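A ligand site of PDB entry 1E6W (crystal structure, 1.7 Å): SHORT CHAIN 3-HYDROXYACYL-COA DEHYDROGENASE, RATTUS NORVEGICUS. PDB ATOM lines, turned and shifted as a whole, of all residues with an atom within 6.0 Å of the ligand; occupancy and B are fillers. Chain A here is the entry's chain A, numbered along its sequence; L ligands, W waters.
Water W2 lies within hydrogen-bond range of O9 of the ligand, N of Gly 22, O of Ser 19, O of Gly 16 and N of Leu 21. Water W1 lies within hydrogen-bond range of O of Gly 92 (2.8 Å) and O1 of the ligand (3.0 Å). Water W5 lies within hydrogen-bond range of the side-chain hydroxyl (OG) of Ser 154, the backbone carbonyl oxygen (O) of Gly 198 and the backbone carbonyl oxygen (O) of Pro 197.
OG of Ser 19 lies within hydrogen-bond range of O2 of the ligand (2.7 Å). The side-chain amino group (NZ) of Lys 171 lies within hydrogen-bond range of an oxygen (O12) of the ligand. OG1 of Thr 202 is in hydrogen-bond range of O8 of the ligand (2.5 Å). N of Leu 21 lies within hydrogen-bond range of O9 of the ligand, 2.7 Å away. N7 of the ligand is in hydrogen-bond range of O of Phe 200, at 3.4 Å. O of Cys 90 sits close to O12 of the ligand (3.1 Å). A nitrogen (N3) of the ligand sits at hydrogen-bond distance from the side-chain amide oxygen (OD1) of Asn 63, at 3.0 Å. N of Phe 200 is in hydrogen-bond range of O14 of the ligand, 2.9 Å away. The backbone NH (N) of Val 64 lies within hydrogen-bond range of a nitrogen (N4) of the ligand. O6 of the ligand is in hydrogen-bond range of OD1 of Asp 40, at 2.6 Å. OH of Tyr 167 is in hydrogen-bond range of O13 of the ligand, 2.6 Å away.
The side-chain sulfur (SG) of Cys 90 lies within hydrogen-bond range of the side-chain hydroxyl (OG1) of Thr 152 (3.7 Å). The backbone NH (N) of Gly 16 sits at hydrogen-bond distance from the backbone carbonyl oxygen (O) of Leu 39 (2.7 Å). OD2 of Asp 40 lies within hydrogen-bond range of N of Ala 18 (3.0 Å). The side-chain sulfur (SG) of Cys 90 lies close to the backbone NH (N) of Gly 22, at 3.8 Å. OD2 of Asp 40 sits at hydrogen-bond distance from N of Gly 17. N of Leu 204 sits close to OG1 of Thr 202 (3.2 Å). The backbone NH (N) of Ala 91 sits at hydrogen-bond distance from the side-chain hydroxyl (OG1) of Thr 15, 2.9 Å away. OD1 of Asn 120 lies within hydrogen-bond range of N of Ile 93 (2.8 Å).
Gly 16 touches the ligand. CA of Gly 20 touches O9 of the ligand (3.3 Å). CG1 of Val 41 touches N4 of the ligand, at 3.7 Å. Ala 62 touches the ligand. Ala 91 touches the ligand (CA to O4, 3.5 Å). Gly 92 touches the ligand (O to C6, 3.5 Å). Ile 93 touches the ligand (CG2 to N2, 3.9 Å). Val 119 touches the ligand. CG2 of Thr 152 touches O11 of the ligand, 3.5 Å away. O of Ala 153 touches C21 of the ligand (3.4 Å). OG of Ser 154 touches C20 of the ligand, at 3.9 Å. Pro 197 touches the ligand (O to C20, 3.5 Å). O of Gly 198 touches C19 of the ligand, 3.2 Å away. CA of Leu 199 touches O14 of the ligand (3.6 Å). Pro 203 touches the ligand (CD to O2, 3.3 Å). Leu 204 touches the ligand. Leu 205 touches the ligand.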
ATOM      1  N   THR A  15      19.534  -3.200  -0.431  1.00  0.00           N
ATOM      2  CA  THR A  15      19.308  -3.309   1.075  1.00  0.00           C
ATOM      3  C   THR A  15      19.234  -4.788   1.363  1.00  0.00           C
ATOM      4  O   THR A  15      18.890  -5.641   0.543  1.00  0.00           O
ATOM      5  CB  THR A  15      18.085  -2.618   1.645  1.00  0.00           C
ATOM      6  OG1 THR A  15      16.883  -3.372   1.308  1.00  0.00           O
ATOM      7  CG2 THR A  15      17.944  -1.252   0.905  1.00  0.00           C
ATOM      8  N   GLY A  16      19.663  -5.118   2.661  1.00  0.00           N
ATOM      9  CA  GLY A  16      19.775  -6.556   2.895  1.00  0.00           C
ATOM     10  C   GLY A  16      20.835  -7.288   2.165  1.00  0.00           C
ATOM     11  O   GLY A  16      20.908  -8.533   1.992  1.00  0.00           O
ATOM     12  N   GLY A  17      21.853  -6.513   1.720  1.00  0.00           N
ATOM     13  CA  GLY A  17      22.885  -7.021   0.875  1.00  0.00           C
ATOM     14  C   GLY A  17      23.984  -7.883   1.495  1.00  0.00           C
ATOM     15  O   GLY A  17      24.797  -8.531   0.719  1.00  0.00           O
ATOM     16  N   ALA A  18      23.995  -7.971   2.851  1.00  0.00           N
ATOM     17  CA  ALA A  18      24.954  -8.914   3.459  1.00  0.00           C
ATOM     18  C   ALA A  18      24.676 -10.379   3.446  1.00  0.00           C
ATOM     19  O   ALA A  18      25.595 -11.206   3.712  1.00  0.00           O
ATOM     20  CB  ALA A  18      25.100  -8.500   4.982  1.00  0.00           C
ATOM     21  N   SER A  19      23.434 -10.832   3.055  1.00  0.00           N
ATOM     22  CA  SER A  19      23.126 -12.279   3.113  1.00  0.00           C
ATOM     23  C   SER A  19      22.014 -12.620   2.097  1.00  0.00           C
ATOM     24  O   SER A  19      21.411 -11.705   1.591  1.00  0.00           O
ATOM     25  CB  SER A  19      22.529 -12.465   4.609  1.00  0.00           C
ATOM     26  OG  SER A  19      22.049 -13.743   4.893  1.00  0.00           O
ATOM     27  N   GLY A  20      21.812 -13.902   1.890  1.00  0.00           N
ATOM     28  CA  GLY A  20      20.607 -14.421   1.155  1.00  0.00           C
ATOM     29  C   GLY A  20      20.393 -13.737  -0.194  1.00  0.00           C
ATOM     30  O   GLY A  20      21.310 -13.750  -0.968  1.00  0.00           O
ATOM     31  N   LEU A  21      19.108 -13.375  -0.397  1.00  0.00           N
ATOM     32  CA  LEU A  21      18.766 -12.816  -1.762  1.00  0.00           C
ATOM     33  C   LEU A  21      19.483 -11.555  -2.133  1.00  0.00           C
ATOM     34  O   LEU A  21      19.863 -11.454  -3.304  1.00  0.00           O
ATOM     35  CB  LEU A  21      17.235 -12.548  -1.708  1.00  0.00           C
ATOM     36  CG  LEU A  21      16.381 -13.836  -1.465  1.00  0.00           C
ATOM     37  CD1 LEU A  21      14.858 -13.553  -1.680  1.00  0.00           C
ATOM     38  CD2 LEU A  21      16.715 -15.041  -2.285  1.00  0.00           C
ATOM     39  N   GLY A  22      19.655 -10.572  -1.216  1.00  0.00           N
ATOM     40  CA  GLY A  22      20.392  -9.362  -1.539  1.00  0.00           C
ATOM     41  C   GLY A  22      21.866  -9.677  -1.869  1.00  0.00           C
ATOM     42  O   GLY A  22      22.375  -9.105  -2.814  1.00  0.00           O
ATOM     43  N   LEU A  39      23.674  -2.354   1.632  1.00  0.00           N
ATOM     44  CA  LEU A  39      23.148  -1.604   2.733  1.00  0.00           C
ATOM     45  C   LEU A  39      22.572  -2.627   3.698  1.00  0.00           C
ATOM     46  O   LEU A  39      21.649  -3.396   3.313  1.00  0.00           O
ATOM     47  CB  LEU A  39      22.204  -0.524   2.241  1.00  0.00           C
ATOM     48  CG  LEU A  39      21.560   0.508   3.101  1.00  0.00           C
ATOM     49  CD1 LEU A  39      20.933   1.727   2.372  1.00  0.00           C
ATOM     50  CD2 LEU A  39      20.489  -0.084   4.031  1.00  0.00           C
ATOM     51  N   ASP A  40      23.232  -2.773   4.922  1.00  0.00           N
ATOM     52  CA  ASP A  40      22.732  -3.789   5.828  1.00  0.00           C
ATOM     53  C   ASP A  40      23.235  -3.253   7.253  1.00  0.00           C
ATOM     54  O   ASP A  40      23.913  -2.197   7.333  1.00  0.00           O
ATOM     55  CB  ASP A  40      23.289  -5.114   5.535  1.00  0.00           C
ATOM     56  CG  ASP A  40      22.465  -6.322   5.938  1.00  0.00           C
ATOM     57  OD1 ASP A  40      22.044  -6.453   7.113  1.00  0.00           O
ATOM     58  OD2 ASP A  40      22.186  -7.176   5.061  1.00  0.00           O
ATOM     59  N   VAL A  41      22.645  -3.811   8.259  1.00  0.00           N
ATOM     60  CA  VAL A  41      23.035  -3.376   9.661  1.00  0.00           C
ATOM     61  C   VAL A  41      24.509  -3.639   9.911  1.00  0.00           C
ATOM     62  O   VAL A  41      25.167  -4.581   9.444  1.00  0.00           O
ATOM     63  CB  VAL A  41      22.208  -4.238  10.670  1.00  0.00           C
ATOM     64  CG1 VAL A  41      20.727  -3.905  10.483  1.00  0.00           C
ATOM     65  CG2 VAL A  41      22.342  -5.731  10.675  1.00  0.00           C
ATOM     66  N   SER A  44      26.291  -7.369  10.718  1.00  0.00           N
ATOM     67  CA  SER A  44      26.159  -8.376   9.723  1.00  0.00           C
ATOM     68  C   SER A  44      27.529  -8.711   9.180  1.00  0.00           C
ATOM     69  O   SER A  44      28.576  -8.096   9.529  1.00  0.00           O
ATOM     70  CB  SER A  44      25.161  -7.762   8.691  1.00  0.00           C
ATOM     71  OG  SER A  44      26.013  -6.870   7.994  1.00  0.00           O
ATOM     72  N   ALA A  62      23.626   0.653   7.530  1.00  0.00           N
ATOM     73  CA  ALA A  62      22.463   1.425   7.774  1.00  0.00           C
ATOM     74  C   ALA A  62      21.279   0.514   8.165  1.00  0.00           C
ATOM     75  O   ALA A  62      21.255  -0.596   7.643  1.00  0.00           O
ATOM     76  CB  ALA A  62      22.051   2.145   6.469  1.00  0.00           C
ATOM     77  N   ASN A  63      20.496   0.985   9.154  1.00  0.00           N
ATOM     78  CA  ASN A  63      19.241   0.243   9.389  1.00  0.00           C
ATOM     79  C   ASN A  63      18.192   0.944   8.602  1.00  0.00           C
ATOM     80  O   ASN A  63      18.044   2.197   8.646  1.00  0.00           O
ATOM     81  CB  ASN A  63      19.029   0.496  10.938  1.00  0.00           C
ATOM     82  CG  ASN A  63      17.776  -0.287  11.404  1.00  0.00           C
ATOM     83  OD1 ASN A  63      16.714  -0.254  10.807  1.00  0.00           O
ATOM     84  ND2 ASN A  63      18.063  -1.232  12.309  1.00  0.00           N
ATOM     85  N   VAL A  64      17.365   0.215   7.744  1.00  0.00           N
ATOM     86  CA  VAL A  64      16.383   0.871   6.854  1.00  0.00           C
ATOM     87  C   VAL A  64      15.245   1.548   7.545  1.00  0.00           C
ATOM     88  O   VAL A  64      14.572   2.317   6.886  1.00  0.00           O
ATOM     89  CB  VAL A  64      15.825  -0.198   5.821  1.00  0.00           C
ATOM     90  CG1 VAL A  64      16.930  -0.725   4.931  1.00  0.00           C
ATOM     91  CG2 VAL A  64      15.099  -1.247   6.651  1.00  0.00           C
ATOM     92  N   THR A  65      15.101   1.461   8.914  1.00  0.00           N
ATOM     93  CA  THR A  65      14.017   2.158   9.560  1.00  0.00           C
ATOM     94  C   THR A  65      14.533   3.593   9.928  1.00  0.00           C
ATOM     95  O   THR A  65      13.725   4.397  10.267  1.00  0.00           O
ATOM     96  CB  THR A  65      13.463   1.433  10.797  1.00  0.00           C
ATOM     97  OG1 THR A  65      14.526   1.273  11.772  1.00  0.00           O
ATOM     98  CG2 THR A  65      13.082  -0.027  10.373  1.00  0.00           C
ATOM     99  N   ASN A  89      15.261  -3.625  -2.791  1.00  0.00           N
ATOM    100  CA  ASN A  89      14.947  -3.674  -1.360  1.00  0.00           C
ATOM    101  C   ASN A  89      14.886  -5.138  -0.915  1.00  0.00           C
ATOM    102  O   ASN A  89      13.843  -5.780  -1.353  1.00  0.00           O
ATOM    103  CB  ASN A  89      13.619  -3.034  -1.024  1.00  0.00           C
ATOM    104  CG  ASN A  89      13.738  -1.542  -1.041  1.00  0.00           C
ATOM    105  OD1 ASN A  89      14.342  -0.937  -0.090  1.00  0.00           O
ATOM    106  ND2 ASN A  89      13.135  -0.830  -1.985  1.00  0.00           N
ATOM    107  N   CYS A  90      15.835  -5.690  -0.210  1.00  0.00           N
ATOM    108  CA  CYS A  90      15.810  -7.096   0.261  1.00  0.00           C
ATOM    109  C   CYS A  90      15.866  -7.159   1.820  1.00  0.00           C
ATOM    110  O   CYS A  90      15.460  -8.162   2.378  1.00  0.00           O
ATOM    111  CB  CYS A  90      16.889  -8.069  -0.231  1.00  0.00           C
ATOM    112  SG  CYS A  90      16.919  -8.153  -2.088  1.00  0.00           S
ATOM    113  N   ALA A  91      16.172  -5.964   2.466  1.00  0.00           N
ATOM    114  CA  ALA A  91      16.147  -6.055   3.943  1.00  0.00           C
ATOM    115  C   ALA A  91      14.798  -6.547   4.451  1.00  0.00           C
ATOM    116  O   ALA A  91      13.722  -5.964   4.122  1.00  0.00           O
ATOM    117  CB  ALA A  91      16.428  -4.556   4.497  1.00  0.00           C
ATOM    118  N   GLY A  92      14.808  -7.496   5.364  1.00  0.00           N
ATOM    119  CA  GLY A  92      13.456  -7.894   5.907  1.00  0.00           C
ATOM    120  C   GLY A  92      13.695  -8.864   7.064  1.00  0.00           C
ATOM    121  O   GLY A  92      14.776  -9.432   7.257  1.00  0.00           O
ATOM    122  N   ILE A  93      12.627  -9.081   7.829  1.00  0.00           N
ATOM    123  CA  ILE A  93      12.632  -9.988   8.967  1.00  0.00           C
ATOM    124  C   ILE A  93      11.333 -10.870   8.862  1.00  0.00           C
ATOM    125  O   ILE A  93      10.373 -10.436   8.239  1.00  0.00           O
ATOM    126  CB  ILE A  93      12.692  -9.296  10.365  1.00  0.00           C
ATOM    127  CG1 ILE A  93      11.746  -8.083  10.484  1.00  0.00           C
ATOM    128  CG2 ILE A  93      14.169  -8.754  10.574  1.00  0.00           C
ATOM    129  CD1 ILE A  93      11.554  -7.648  11.984  1.00  0.00           C
ATOM    130  N   ALA A  94      11.282 -11.898   9.669  1.00  0.00           N
ATOM    131  CA  ALA A  94      10.100 -12.776   9.648  1.00  0.00           C
ATOM    132  C   ALA A  94       9.836 -13.339  11.048  1.00  0.00           C
ATOM    133  O   ALA A  94      10.816 -13.421  11.774  1.00  0.00           O
ATOM    134  CB  ALA A  94      10.334 -13.974   8.732  1.00  0.00           C
ATOM    135  N   VAL A 119      10.264  -2.781   9.888  1.00  0.00           N
ATOM    136  CA  VAL A 119      11.398  -3.132   9.075  1.00  0.00           C
ATOM    137  C   VAL A 119      10.942  -3.329   7.587  1.00  0.00           C
ATOM    138  O   VAL A 119      11.633  -2.955   6.679  1.00  0.00           O
ATOM    139  CB  VAL A 119      12.066  -4.336   9.665  1.00  0.00           C
ATOM    140  CG1 VAL A 119      13.254  -4.717   8.745  1.00  0.00           C
ATOM    141  CG2 VAL A 119      12.566  -4.135  11.133  1.00  0.00           C
ATOM    142  N   ASN A 120      10.017  -4.264   7.458  1.00  0.00           N
ATOM    143  CA  ASN A 120       9.629  -4.739   6.096  1.00  0.00           C
ATOM    144  C   ASN A 120       8.932  -3.678   5.282  1.00  0.00           C
ATOM    145  O   ASN A 120       9.257  -3.614   4.066  1.00  0.00           O
ATOM    146  CB  ASN A 120       8.721  -5.969   6.321  1.00  0.00           C
ATOM    147  CG  ASN A 120       9.492  -7.130   6.745  1.00  0.00           C
ATOM    148  OD1 ASN A 120      10.720  -7.188   7.101  1.00  0.00           O
ATOM    149  ND2 ASN A 120       8.889  -8.380   6.804  1.00  0.00           N
ATOM    150  N   THR A 152      11.103  -6.410  -2.580  1.00  0.00           N
ATOM    151  CA  THR A 152      10.837  -7.886  -2.445  1.00  0.00           C
ATOM    152  C   THR A 152       9.664  -8.053  -1.479  1.00  0.00           C
ATOM    153  O   THR A 152       9.664  -7.618  -0.317  1.00  0.00           O
ATOM    154  CB  THR A 152      12.039  -8.503  -1.685  1.00  0.00           C
ATOM    155  OG1 THR A 152      13.199  -8.193  -2.394  1.00  0.00           O
ATOM    156  CG2 THR A 152      11.786 -10.049  -1.753  1.00  0.00           C
ATOM    157  N   ALA A 153       8.514  -8.541  -2.014  1.00  0.00           N
ATOM    158  CA  ALA A 153       7.377  -8.923  -1.178  1.00  0.00           C
ATOM    159  C   ALA A 153       7.500 -10.418  -0.821  1.00  0.00           C
ATOM    160  O   ALA A 153       8.544 -10.781  -0.224  1.00  0.00           O
ATOM    161  CB  ALA A 153       6.135  -8.638  -1.930  1.00  0.00           C
ATOM    162  N   SER A 154       6.503 -11.211  -1.113  1.00  0.00           N
ATOM    163  CA  SER A 154       6.490 -12.612  -0.790  1.00  0.00           C
ATOM    164  C   SER A 154       5.146 -13.177  -1.297  1.00  0.00           C
ATOM    165  O   SER A 154       4.145 -12.507  -1.281  1.00  0.00           O
ATOM    166  CB  SER A 154       6.422 -12.657   0.817  1.00  0.00           C
ATOM    167  OG  SER A 154       6.314 -14.095   1.120  1.00  0.00           O
ATOM    168  N   VAL A 155       5.174 -14.542  -1.457  1.00  0.00           N
ATOM    169  CA  VAL A 155       3.858 -15.135  -1.761  1.00  0.00           C
ATOM    170  C   VAL A 155       2.947 -14.996  -0.566  1.00  0.00           C
ATOM    171  O   VAL A 155       1.682 -15.141  -0.661  1.00  0.00           O
ATOM    172  CB  VAL A 155       3.927 -16.568  -2.287  1.00  0.00           C
ATOM    173  CG1 VAL A 155       4.615 -16.593  -3.662  1.00  0.00           C
ATOM    174  CG2 VAL A 155       4.684 -17.514  -1.310  1.00  0.00           C
ATOM    175  N   TYR A 167       3.829 -10.804   8.972  1.00  0.00           N
ATOM    176  CA  TYR A 167       4.685 -10.852   7.801  1.00  0.00           C
ATOM    177  C   TYR A 167       3.830 -10.656   6.544  1.00  0.00           C
ATOM    178  O   TYR A 167       4.134  -9.783   5.720  1.00  0.00           O
ATOM    179  CB  TYR A 167       5.397 -12.220   7.786  1.00  0.00           C
ATOM    180  CG  TYR A 167       6.373 -12.459   6.604  1.00  0.00           C
ATOM    181  CD1 TYR A 167       7.629 -11.794   6.674  1.00  0.00           C
ATOM    182  CD2 TYR A 167       6.081 -13.231   5.487  1.00  0.00           C
ATOM    183  CE1 TYR A 167       8.597 -12.067   5.670  1.00  0.00           C
ATOM    184  CE2 TYR A 167       7.055 -13.498   4.489  1.00  0.00           C
ATOM    185  CZ  TYR A 167       8.292 -12.848   4.616  1.00  0.00           C
ATOM    186  OH  TYR A 167       9.319 -12.998   3.693  1.00  0.00           O
ATOM    187  N   LYS A 171       4.056  -7.628   3.757  1.00  0.00           N
ATOM    188  CA  LYS A 171       4.360  -7.871   2.352  1.00  0.00           C
ATOM    189  C   LYS A 171       3.170  -7.394   1.539  1.00  0.00           C
ATOM    190  O   LYS A 171       3.384  -7.061   0.314  1.00  0.00           O
ATOM    191  CB  LYS A 171       4.641  -9.405   2.172  1.00  0.00           C
ATOM    192  CG  LYS A 171       5.983  -9.728   2.867  1.00  0.00           C
ATOM    193  CD  LYS A 171       7.223  -8.866   2.653  1.00  0.00           C
ATOM    194  CE  LYS A 171       8.497  -9.571   3.085  1.00  0.00           C
ATOM    195  NZ  LYS A 171       9.696  -8.902   2.507  1.00  0.00           N
ATOM    196  N   ALA A 196       7.858 -11.335  -5.726  1.00  0.00           N
ATOM    197  CA  ALA A 196       7.224 -12.068  -4.612  1.00  0.00           C
ATOM    198  C   ALA A 196       7.743 -13.533  -4.580  1.00  0.00           C
ATOM    199  O   ALA A 196       7.230 -14.410  -5.270  1.00  0.00           O
ATOM    200  CB  ALA A 196       5.736 -12.209  -4.676  1.00  0.00           C
ATOM    201  N   PRO A 197       8.875 -13.737  -3.899  1.00  0.00           N
ATOM    202  CA  PRO A 197       9.451 -15.061  -3.879  1.00  0.00           C
ATOM    203  C   PRO A 197       8.571 -16.007  -3.093  1.00  0.00           C
ATOM    204  O   PRO A 197       7.833 -15.653  -2.107  1.00  0.00           O
ATOM    205  CB  PRO A 197      10.840 -14.915  -3.105  1.00  0.00           C
ATOM    206  CG  PRO A 197      11.049 -13.425  -3.151  1.00  0.00           C
ATOM    207  CD  PRO A 197       9.630 -12.768  -3.084  1.00  0.00           C
ATOM    208  N   GLY A 198       8.773 -17.310  -3.466  1.00  0.00           N
ATOM    209  CA  GLY A 198       8.042 -18.300  -2.768  1.00  0.00           C
ATOM    210  C   GLY A 198       9.074 -18.751  -1.612  1.00  0.00           C
ATOM    211  O   GLY A 198       8.836 -18.257  -0.534  1.00  0.00           O
ATOM    212  N   LEU A 199       9.483 -19.969  -1.642  1.00  0.00           N
ATOM    213  CA  LEU A 199      10.463 -20.398  -0.561  1.00  0.00           C
ATOM    214  C   LEU A 199      11.854 -20.569  -1.193  1.00  0.00           C
ATOM    215  O   LEU A 199      11.980 -21.478  -2.088  1.00  0.00           O
ATOM    216  CB  LEU A 199       9.973 -21.722  -0.030  1.00  0.00           C
ATOM    217  CG  LEU A 199       8.564 -21.924   0.444  1.00  0.00           C
ATOM    218  CD1 LEU A 199       8.130 -23.370   0.665  1.00  0.00           C
ATOM    219  CD2 LEU A 199       8.456 -21.071   1.696  1.00  0.00           C
ATOM    220  N   PHE A 200      12.850 -19.984  -0.546  1.00  0.00           N
ATOM    221  CA  PHE A 200      14.208 -19.921  -1.016  1.00  0.00           C
ATOM    222  C   PHE A 200      15.217 -20.403   0.069  1.00  0.00           C
ATOM    223  O   PHE A 200      14.930 -20.114   1.256  1.00  0.00           O
ATOM    224  CB  PHE A 200      14.565 -18.424  -1.391  1.00  0.00           C
ATOM    225  CG  PHE A 200      14.269 -18.175  -2.832  1.00  0.00           C
ATOM    226  CD1 PHE A 200      12.883 -18.076  -3.215  1.00  0.00           C
ATOM    227  CD2 PHE A 200      15.189 -18.134  -3.855  1.00  0.00           C
ATOM    228  CE1 PHE A 200      12.566 -17.889  -4.565  1.00  0.00           C
ATOM    229  CE2 PHE A 200      14.883 -17.901  -5.210  1.00  0.00           C
ATOM    230  CZ  PHE A 200      13.531 -17.839  -5.594  1.00  0.00           C
ATOM    231  N   ALA A 201      16.280 -20.967  -0.470  1.00  0.00           N
ATOM    232  CA  ALA A 201      17.334 -21.470   0.529  1.00  0.00           C
ATOM    233  C   ALA A 201      18.173 -20.335   1.030  1.00  0.00           C
ATOM    234  O   ALA A 201      19.205 -20.094   0.393  1.00  0.00           O
ATOM    235  CB  ALA A 201      18.079 -22.444  -0.362  1.00  0.00           C
ATOM    236  N   THR A 202      17.734 -19.661   2.055  1.00  0.00           N
ATOM    237  CA  THR A 202      18.522 -18.562   2.636  1.00  0.00           C
ATOM    238  C   THR A 202      18.587 -18.801   4.167  1.00  0.00           C
ATOM    239  O   THR A 202      17.833 -19.611   4.717  1.00  0.00           O
ATOM    240  CB  THR A 202      17.956 -17.162   2.390  1.00  0.00           C
ATOM    241  OG1 THR A 202      16.751 -16.984   3.174  1.00  0.00           O
ATOM    242  CG2 THR A 202      17.675 -16.984   0.915  1.00  0.00           C
ATOM    243  N   PRO A 203      19.331 -17.955   4.847  1.00  0.00           N
ATOM    244  CA  PRO A 203      19.427 -18.042   6.327  1.00  0.00           C
ATOM    245  C   PRO A 203      18.115 -17.711   7.014  1.00  0.00           C
ATOM    246  O   PRO A 203      18.021 -17.983   8.221  1.00  0.00           O
ATOM    247  CB  PRO A 203      20.567 -17.116   6.683  1.00  0.00           C
ATOM    248  CG  PRO A 203      21.438 -17.056   5.491  1.00  0.00           C
ATOM    249  CD  PRO A 203      20.418 -17.080   4.326  1.00  0.00           C
ATOM    250  N   LEU A 204      17.074 -17.200   6.385  1.00  0.00           N
ATOM    251  CA  LEU A 204      15.688 -17.396   6.804  1.00  0.00           C
ATOM    252  C   LEU A 204      15.261 -18.869   6.805  1.00  0.00           C
ATOM    253  O   LEU A 204      14.881 -19.247   7.916  1.00  0.00           O
ATOM    254  CB  LEU A 204      14.999 -16.454   5.808  1.00  0.00           C
ATOM    255  CG  LEU A 204      13.885 -15.500   6.213  1.00  0.00           C
ATOM    256  CD1 LEU A 204      14.447 -14.249   6.875  1.00  0.00           C
ATOM    257  CD2 LEU A 204      12.955 -14.962   5.107  1.00  0.00           C
ATOM    258  N   LEU A 205      15.284 -19.713   5.791  1.00  0.00           N
ATOM    259  CA  LEU A 205      14.881 -21.100   5.746  1.00  0.00           C
ATOM    260  C   LEU A 205      15.971 -22.041   6.255  1.00  0.00           C
ATOM    261  O   LEU A 205      15.920 -22.492   7.417  1.00  0.00           O
ATOM    262  CB  LEU A 205      14.281 -21.577   4.408  1.00  0.00           C
ATOM    263  CG  LEU A 205      12.942 -21.074   3.967  1.00  0.00           C
ATOM    264  CD1 LEU A 205      12.582 -19.653   4.322  1.00  0.00           C
ATOM    265  CD2 LEU A 205      12.585 -21.448   2.554  1.00  0.00           C
HETATM  266  P1  LIG L   1      18.355 -12.998   5.062  1.00  0.00           P
HETATM  267  O1  LIG L   1      18.109 -13.039   6.536  1.00  0.00           O
HETATM  268  O2  LIG L   1      19.377 -13.974   4.582  1.00  0.00           O
HETATM  269  O3  LIG L   1      18.752 -11.564   4.539  1.00  0.00           O
HETATM  270  C1  LIG L   1      18.055 -10.407   5.026  1.00  0.00           C
HETATM  271  C2  LIG L   1      19.113  -9.282   5.227  1.00  0.00           C
HETATM  272  O4  LIG L   1      18.327  -8.212   5.613  1.00  0.00           O
HETATM  273  C3  LIG L   1      19.967  -9.760   6.470  1.00  0.00           C
HETATM  274  O5  LIG L   1      21.343  -9.466   6.012  1.00  0.00           O
HETATM  275  C4  LIG L   1      19.568  -8.741   7.490  1.00  0.00           C
HETATM  276  O6  LIG L   1      20.720  -8.262   8.350  1.00  0.00           O
HETATM  277  C5  LIG L   1      19.072  -7.506   6.666  1.00  0.00           C
HETATM  278  N1  LIG L   1      18.110  -6.776   7.528  1.00  0.00           N
HETATM  279  C6  LIG L   1      17.121  -7.127   8.403  1.00  0.00           C
HETATM  280  N2  LIG L   1      16.565  -6.083   8.996  1.00  0.00           N
HETATM  281  C7  LIG L   1      17.272  -4.968   8.568  1.00  0.00           C
HETATM  282  C8  LIG L   1      17.178  -3.614   8.853  1.00  0.00           C
HETATM  283  N3  LIG L   1      16.289  -2.974   9.688  1.00  0.00           N
HETATM  284  N4  LIG L   1      18.033  -2.766   8.182  1.00  0.00           N
HETATM  285  C9  LIG L   1      18.904  -3.257   7.206  1.00  0.00           C
HETATM  286  N5  LIG L   1      19.086  -4.556   6.929  1.00  0.00           N
HETATM  287  C10 LIG L   1      18.204  -5.355   7.633  1.00  0.00           C
HETATM  288  O7  LIG L   1      16.915 -13.268   4.369  1.00  0.00           O
HETATM  289  P2  LIG L   1      16.533 -13.338   2.791  1.00  0.00           P
HETATM  290  O8  LIG L   1      15.864 -14.659   2.683  1.00  0.00           O
HETATM  291  O9  LIG L   1      17.675 -13.133   1.876  1.00  0.00           O
HETATM  292  O10 LIG L   1      15.450 -12.162   2.732  1.00  0.00           O
HETATM  293  C11 LIG L   1      15.556 -11.179   1.683  1.00  0.00           C
HETATM  294  C12 LIG L   1      14.129 -10.689   1.377  1.00  0.00           C
HETATM  295  O11 LIG L   1      13.351 -11.823   0.841  1.00  0.00           O
HETATM  296  C13 LIG L   1      13.324 -10.338   2.670  1.00  0.00           C
HETATM  297  O12 LIG L   1      12.560  -9.206   2.399  1.00  0.00           O
HETATM  298  C14 LIG L   1      12.477 -11.580   2.930  1.00  0.00           C
HETATM  299  O13 LIG L   1      11.171 -11.208   3.546  1.00  0.00           O
HETATM  300  C15 LIG L   1      12.110 -11.960   1.461  1.00  0.00           C
HETATM  301  N6  LIG L   1      11.719 -13.420   1.198  1.00  0.00           N
HETATM  302  C16 LIG L   1      12.510 -14.430   1.530  1.00  0.00           C
HETATM  303  C17 LIG L   1      12.045 -15.729   1.276  1.00  0.00           C
HETATM  304  C18 LIG L   1      12.777 -17.042   1.588  1.00  0.00           C
HETATM  305  O14 LIG L   1      12.206 -18.124   1.542  1.00  0.00           O
HETATM  306  N7  LIG L   1      14.066 -16.858   1.913  1.00  0.00           N
HETATM  307  C19 LIG L   1      10.763 -16.051   0.678  1.00  0.00           C
HETATM  308  C20 LIG L   1      10.075 -14.848   0.413  1.00  0.00           C
HETATM  309  C21 LIG L   1      10.427 -13.504   0.621  1.00  0.00           C
HETATM  310  O   HOH W   1      16.764 -11.043   8.265  1.00  0.00           O
HETATM  311  O   HOH W   2      18.721 -10.524   1.507  1.00  0.00           O
HETATM  312  O   HOH W   3      22.891 -10.497   7.959  1.00  0.00           O
HETATM  313  O   HOH W   4      12.783  -6.722   1.514  1.00  0.00           O
HETATM  314  O   HOH W   5       7.298 -16.541   1.158  1.00  0.00           O
HETATM  315  O   HOH W   6      19.542 -13.910   8.576  1.00  0.00           O
HETATM  316  O   HOH W   7      16.049  -5.645  11.789  1.00  0.00           O
HETATM  317  O   HOH W   8      19.593  -8.150  11.043  1.00  0.00           O
HETATM  318  O   HOH W   9       9.136 -15.906   3.637  1.00  0.00           O
